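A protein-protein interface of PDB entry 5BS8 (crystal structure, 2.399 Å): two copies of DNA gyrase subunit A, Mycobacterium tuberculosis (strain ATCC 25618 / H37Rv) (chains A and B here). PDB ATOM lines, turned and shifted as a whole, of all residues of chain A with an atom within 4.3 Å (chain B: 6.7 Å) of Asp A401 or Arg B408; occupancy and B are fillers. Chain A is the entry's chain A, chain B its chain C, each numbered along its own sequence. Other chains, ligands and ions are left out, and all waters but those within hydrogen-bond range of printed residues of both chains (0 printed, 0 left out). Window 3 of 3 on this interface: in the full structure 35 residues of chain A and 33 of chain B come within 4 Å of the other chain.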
ATOM      1  N   ALA A 399     -22.160 -13.593  -6.511  1.00  0.00           N
ATOM      2  CA  ALA A 399     -22.795 -14.451  -7.507  1.00  0.00           C
ATOM      3  C   ALA A 399     -21.760 -14.969  -8.500  1.00  0.00           C
ATOM      4  O   ALA A 399     -21.991 -14.969  -9.708  1.00  0.00           O
ATOM      5  CB  ALA A 399     -23.891 -13.690  -8.231  1.00  0.00           C
ATOM      6  N   LEU A 400     -20.626 -15.423  -7.977  1.00  0.00           N
ATOM      7  CA  LEU A 400     -19.468 -15.769  -8.799  1.00  0.00           C
ATOM      8  C   LEU A 400     -19.725 -16.901  -9.798  1.00  0.00           C
ATOM      9  O   LEU A 400     -19.285 -16.824 -10.947  1.00  0.00           O
ATOM     10  CB  LEU A 400     -18.292 -16.143  -7.895  1.00  0.00           C
ATOM     11  CG  LEU A 400     -16.966 -16.470  -8.585  1.00  0.00           C
ATOM     12  CD1 LEU A 400     -16.524 -15.338  -9.500  1.00  0.00           C
ATOM     13  CD2 LEU A 400     -15.897 -16.757  -7.544  1.00  0.00           C
ATOM     14  N   ASP A 401     -20.419 -17.950  -9.363  1.00  0.00           N
ATOM     15  CA  ASP A 401     -20.732 -19.080 -10.239  1.00  0.00           C
ATOM     16  C   ASP A 401     -21.472 -18.622 -11.492  1.00  0.00           C
ATOM     17  O   ASP A 401     -21.202 -19.094 -12.596  1.00  0.00           O
ATOM     18  CB  ASP A 401     -21.574 -20.125  -9.497  1.00  0.00           C
ATOM     19  CG  ASP A 401     -20.861 -20.708  -8.292  1.00  0.00           C
ATOM     20  OD1 ASP A 401     -19.616 -20.632  -8.234  1.00  0.00           O
ATOM     21  OD2 ASP A 401     -21.550 -21.249  -7.400  1.00  0.00           O
ATOM     22  N   GLU A 402     -22.401 -17.690 -11.310  1.00  0.00           N
ATOM     23  CA  GLU A 402     -23.244 -17.217 -12.400  1.00  0.00           C
ATOM     24  C   GLU A 402     -22.480 -16.315 -13.367  1.00  0.00           C
ATOM     25  O   GLU A 402     -22.705 -16.362 -14.577  1.00  0.00           O
ATOM     26  CB  GLU A 402     -24.454 -16.472 -11.835  1.00  0.00           C
ATOM     27  CG  GLU A 402     -25.252 -17.289 -10.834  1.00  0.00           C
ATOM     28  CD  GLU A 402     -26.483 -16.563 -10.332  1.00  0.00           C
ATOM     29  OE1 GLU A 402     -26.367 -15.377  -9.957  1.00  0.00           O
ATOM     30  OE2 GLU A 402     -27.572 -17.178 -10.317  1.00  0.00           O
ATOM     31  N   VAL A 403     -21.581 -15.497 -12.826  1.00  0.00           N
ATOM     32  CA  VAL A 403     -20.795 -14.557 -13.624  1.00  0.00           C
ATOM     33  C   VAL A 403     -20.061 -15.267 -14.760  1.00  0.00           C
ATOM     34  O   VAL A 403     -20.161 -14.868 -15.920  1.00  0.00           O
ATOM     35  CB  VAL A 403     -19.764 -13.799 -12.743  1.00  0.00           C
ATOM     36  CG1 VAL A 403     -18.765 -13.009 -13.595  1.00  0.00           C
ATOM     37  CG2 VAL A 403     -20.474 -12.865 -11.780  1.00  0.00           C
ATOM     38  N   ILE A 404     -19.333 -16.322 -14.417  1.00  0.00           N
ATOM     39  CA  ILE A 404     -18.493 -17.025 -15.379  1.00  0.00           C
ATOM     40  C   ILE A 404     -19.318 -17.669 -16.487  1.00  0.00           C
ATOM     41  O   ILE A 404     -19.019 -17.488 -17.667  1.00  0.00           O
ATOM     42  CB  ILE A 404     -17.642 -18.101 -14.678  1.00  0.00           C
ATOM     43  CG1 ILE A 404     -16.700 -17.424 -13.677  1.00  0.00           C
ATOM     44  CG2 ILE A 404     -16.849 -18.930 -15.701  1.00  0.00           C
ATOM     45  CD1 ILE A 404     -15.876 -18.373 -12.853  1.00  0.00           C
ATOM     46  N   ALA A 405     -20.351 -18.413 -16.102  1.00  0.00           N
ATOM     47  CA  ALA A 405     -21.191 -19.125 -17.059  1.00  0.00           C
ATOM     48  C   ALA A 405     -21.729 -18.182 -18.129  1.00  0.00           C
ATOM     49  O   ALA A 405     -21.846 -18.551 -19.299  1.00  0.00           O
ATOM     50  CB  ALA A 405     -22.339 -19.812 -16.341  1.00  0.00           C
ATOM     51  N   LEU A 442      -9.442 -14.334  -7.943  1.00  0.00           N
ATOM     52  CA  LEU A 442     -10.480 -15.301  -7.588  1.00  0.00           C
ATOM     53  C   LEU A 442     -10.029 -16.226  -6.453  1.00  0.00           C
ATOM     54  O   LEU A 442     -10.809 -17.044  -5.963  1.00  0.00           O
ATOM     55  CB  LEU A 442     -10.882 -16.128  -8.812  1.00  0.00           C
ATOM     56  CG  LEU A 442     -11.531 -15.356  -9.966  1.00  0.00           C
ATOM     57  CD1 LEU A 442     -11.934 -16.313 -11.079  1.00  0.00           C
ATOM     58  CD2 LEU A 442     -12.741 -14.552  -9.499  1.00  0.00           C
ATOM     59  N   ARG A 447     -10.262 -12.406  -2.892  1.00  0.00           N
ATOM     60  CA  ARG A 447     -11.684 -12.104  -2.794  1.00  0.00           C
ATOM     61  C   ARG A 447     -11.946 -11.312  -1.519  1.00  0.00           C
ATOM     62  O   ARG A 447     -12.686 -10.331  -1.530  1.00  0.00           O
ATOM     63  CB  ARG A 447     -12.521 -13.387  -2.817  1.00  0.00           C
ATOM     64  CG  ARG A 447     -12.531 -14.090  -4.166  1.00  0.00           C
ATOM     65  CD  ARG A 447     -13.478 -15.283  -4.194  1.00  0.00           C
ATOM     66  NE  ARG A 447     -12.825 -16.530  -3.786  1.00  0.00           N
ATOM     67  CZ  ARG A 447     -13.091 -17.216  -2.673  1.00  0.00           C
ATOM     68  NH1 ARG A 447     -14.013 -16.802  -1.809  1.00  0.00           N
ATOM     69  NH2 ARG A 447     -12.426 -18.335  -2.424  1.00  0.00           N
ATOM     70  N   VAL B 403      -9.746 -25.776 -13.948  1.00  0.00           N
ATOM     71  CA  VAL B 403      -8.806 -24.687 -13.692  1.00  0.00           C
ATOM     72  C   VAL B 403      -9.418 -23.610 -12.804  1.00  0.00           C
ATOM     73  O   VAL B 403      -8.806 -23.176 -11.828  1.00  0.00           O
ATOM     74  CB  VAL B 403      -8.325 -24.044 -15.017  1.00  0.00           C
ATOM     75  CG1 VAL B 403      -7.635 -22.698 -14.773  1.00  0.00           C
ATOM     76  CG2 VAL B 403      -7.383 -24.986 -15.739  1.00  0.00           C
ATOM     77  N   ILE B 404     -10.623 -23.172 -13.149  1.00  0.00           N
ATOM     78  CA  ILE B 404     -11.299 -22.138 -12.378  1.00  0.00           C
ATOM     79  C   ILE B 404     -11.642 -22.649 -10.984  1.00  0.00           C
ATOM     80  O   ILE B 404     -11.418 -21.957  -9.993  1.00  0.00           O
ATOM     81  CB  ILE B 404     -12.580 -21.657 -13.084  1.00  0.00           C
ATOM     82  CG1 ILE B 404     -12.213 -20.999 -14.417  1.00  0.00           C
ATOM     83  CG2 ILE B 404     -13.351 -20.682 -12.196  1.00  0.00           C
ATOM     84  CD1 ILE B 404     -13.400 -20.582 -15.269  1.00  0.00           C
ATOM     85  N   ALA B 405     -12.196 -23.854 -10.914  1.00  0.00           N
ATOM     86  CA  ALA B 405     -12.503 -24.475  -9.633  1.00  0.00           C
ATOM     87  C   ALA B 405     -11.245 -24.584  -8.774  1.00  0.00           C
ATOM     88  O   ALA B 405     -11.295 -24.401  -7.558  1.00  0.00           O
ATOM     89  CB  ALA B 405     -13.121 -25.844  -9.845  1.00  0.00           C
ATOM     90  N   LEU B 406     -10.118 -24.877  -9.416  1.00  0.00           N
ATOM     91  CA  LEU B 406      -8.841 -24.989  -8.720  1.00  0.00           C
ATOM     92  C   LEU B 406      -8.421 -23.651  -8.119  1.00  0.00           C
ATOM     93  O   LEU B 406      -8.048 -23.580  -6.949  1.00  0.00           O
ATOM     94  CB  LEU B 406      -7.755 -25.496  -9.675  1.00  0.00           C
ATOM     95  CG  LEU B 406      -6.325 -25.539  -9.130  1.00  0.00           C
ATOM     96  CD1 LEU B 406      -6.191 -26.609  -8.062  1.00  0.00           C
ATOM     97  CD2 LEU B 406      -5.332 -25.770 -10.253  1.00  0.00           C
ATOM     98  N   ILE B 407      -8.477 -22.598  -8.930  1.00  0.00           N
ATOM     99  CA  ILE B 407      -8.079 -21.266  -8.489  1.00  0.00           C
ATOM    100  C   ILE B 407      -8.978 -20.781  -7.356  1.00  0.00           C
ATOM    101  O   ILE B 407      -8.496 -20.240  -6.362  1.00  0.00           O
ATOM    102  CB  ILE B 407      -8.118 -20.251  -9.657  1.00  0.00           C
ATOM    103  CG1 ILE B 407      -7.050 -20.603 -10.697  1.00  0.00           C
ATOM    104  CG2 ILE B 407      -7.896 -18.823  -9.149  1.00  0.00           C
ATOM    105  CD1 ILE B 407      -7.093 -19.758 -11.965  1.00  0.00           C
ATOM    106  N   ARG B 408     -10.283 -20.977  -7.511  1.00  0.00           N
ATOM    107  CA  ARG B 408     -11.246 -20.513  -6.521  1.00  0.00           C
ATOM    108  C   ARG B 408     -11.029 -21.188  -5.169  1.00  0.00           C
ATOM    109  O   ARG B 408     -11.077 -20.535  -4.127  1.00  0.00           O
ATOM    110  CB  ARG B 408     -12.674 -20.770  -7.004  1.00  0.00           C
ATOM    111  CG  ARG B 408     -13.091 -19.922  -8.196  1.00  0.00           C
ATOM    112  CD  ARG B 408     -14.480 -20.305  -8.662  1.00  0.00           C
ATOM    113  NE  ARG B 408     -15.482 -20.021  -7.640  1.00  0.00           N
ATOM    114  CZ  ARG B 408     -16.711 -20.525  -7.633  1.00  0.00           C
ATOM    115  NH1 ARG B 408     -17.101 -21.355  -8.592  1.00  0.00           N
ATOM    116  NH2 ARG B 408     -17.553 -20.206  -6.659  1.00  0.00           N
ATOM    117  N   ALA B 409     -10.780 -22.492  -5.196  1.00  0.00           N
ATOM    118  CA  ALA B 409     -10.634 -23.271  -3.971  1.00  0.00           C
ATOM    119  C   ALA B 409      -9.267 -23.067  -3.318  1.00  0.00           C
ATOM    120  O   ALA B 409      -9.010 -23.585  -2.231  1.00  0.00           O
ATOM    121  CB  ALA B 409     -10.863 -24.749  -4.261  1.00  0.00           C
ATOM    122  N   SER B 410      -8.396 -22.310  -3.978  1.00  0.00           N
ATOM    123  CA  SER B 410      -7.070 -22.027  -3.439  1.00  0.00           C
ATOM    124  C   SER B 410      -7.125 -20.842  -2.480  1.00  0.00           C
ATOM    125  O   SER B 410      -7.739 -19.818  -2.779  1.00  0.00           O
ATOM    126  CB  SER B 410      -6.079 -21.747  -4.570  1.00  0.00           C
ATOM    127  OG  SER B 410      -6.001 -22.848  -5.457  1.00  0.00           O
ATOM    128  N   GLU B 411      -6.482 -20.988  -1.325  1.00  0.00           N
ATOM    129  CA  GLU B 411      -6.493 -19.937  -0.314  1.00  0.00           C
ATOM    130  C   GLU B 411      -5.651 -18.739  -0.745  1.00  0.00           C
ATOM    131  O   GLU B 411      -5.973 -17.598  -0.417  1.00  0.00           O
ATOM    132  CB  GLU B 411      -5.994 -20.482   1.024  1.00  0.00           C
ATOM    133  CG  GLU B 411      -6.978 -21.424   1.700  1.00  0.00           C
ATOM    134  CD  GLU B 411      -6.501 -21.889   3.060  1.00  0.00           C
ATOM    135  OE1 GLU B 411      -5.351 -21.571   3.428  1.00  0.00           O
ATOM    136  OE2 GLU B 411      -7.279 -22.571   3.761  1.00  0.00           O
ATOM    137  N   ALA B 416      -2.665 -21.631  -5.807  1.00  0.00           N
ATOM    138  CA  ALA B 416      -3.319 -21.803  -7.095  1.00  0.00           C
ATOM    139  C   ALA B 416      -2.292 -22.086  -8.187  1.00  0.00           C
ATOM    140  O   ALA B 416      -2.491 -22.966  -9.023  1.00  0.00           O
ATOM    141  CB  ALA B 416      -4.132 -20.575  -7.441  1.00  0.00           C
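The guanidinium group of Arg B408 lies within salt-bridge range of the side-chain carboxylate of Asp A401 (2.6 Å).
NH2 of Arg A447 is in hydrogen-bond range of O of Arg B408, at 3.1 Å.
The backbone carbonyl oxygen (O) of Leu A442 lies within hydrogen-bond range of the guanidinium group (NE) of Arg A447, at 3.0 Å.
Among the printed residues, merely in contact across the chains: Leu A400 with Arg B408, Ile A404 with Ile B404, Leu A442 with Ile B407 and Leu A442 with Arg B408.
Ala A399 touches none of the printed residues of chain B.
Of the printed residues of chain B, Leu A400 touches Arg B408 (3.3 Å).
Of chain B, only Arg B408 comes within 4 Å of Asp A401.
Of the printed residues of chain B, Ile A404 touches Ile B404 (3.5 Å).
Of the printed residues of chain B, Leu A442 touches Ile B407 (3.97 Å) and Arg B408 (3.5 Å).
Val B403 touches none of the printed residues of chain A.
Of the printed residues of chain A, Ile B404 touches Ile A404.
Of chain A, only Leu A400, Asp A401, Leu A442 and Arg A447 come within 4 Å of Arg B408.
The nearest printed residue of chain A that does not touch Arg B408 is Ile A404 (4.8 Å).
The nearest printed residue of chain B that does not touch Arg A447 is Ser B410 (4.9 Å).
Hydrophobic or aromatic side chains of chain B that line the printed part of chain A: Ile B404.
Along chain B the printed residues that touch a printed residue of chain A span positions 404 to 408.
Hydrophobic or aromatic side chains of chain A that line the printed part of chain B: Leu A400 and Ile A404.
Along chain A the printed residues that touch a printed residue of chain B span positions 400 to 447.
Among the printed residues, Asp or Glu carboxylates within 4 Å of a Lys or Arg side-chain nitrogen of the other chain: Asp A401 with Arg B408 (2.6 Å).
Ile A404 touches its own counterpart, Ile B404.
Of the 6 pairs that touch across the chains among the printed residues, 1 has its exchanged pair printed and touching as well.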
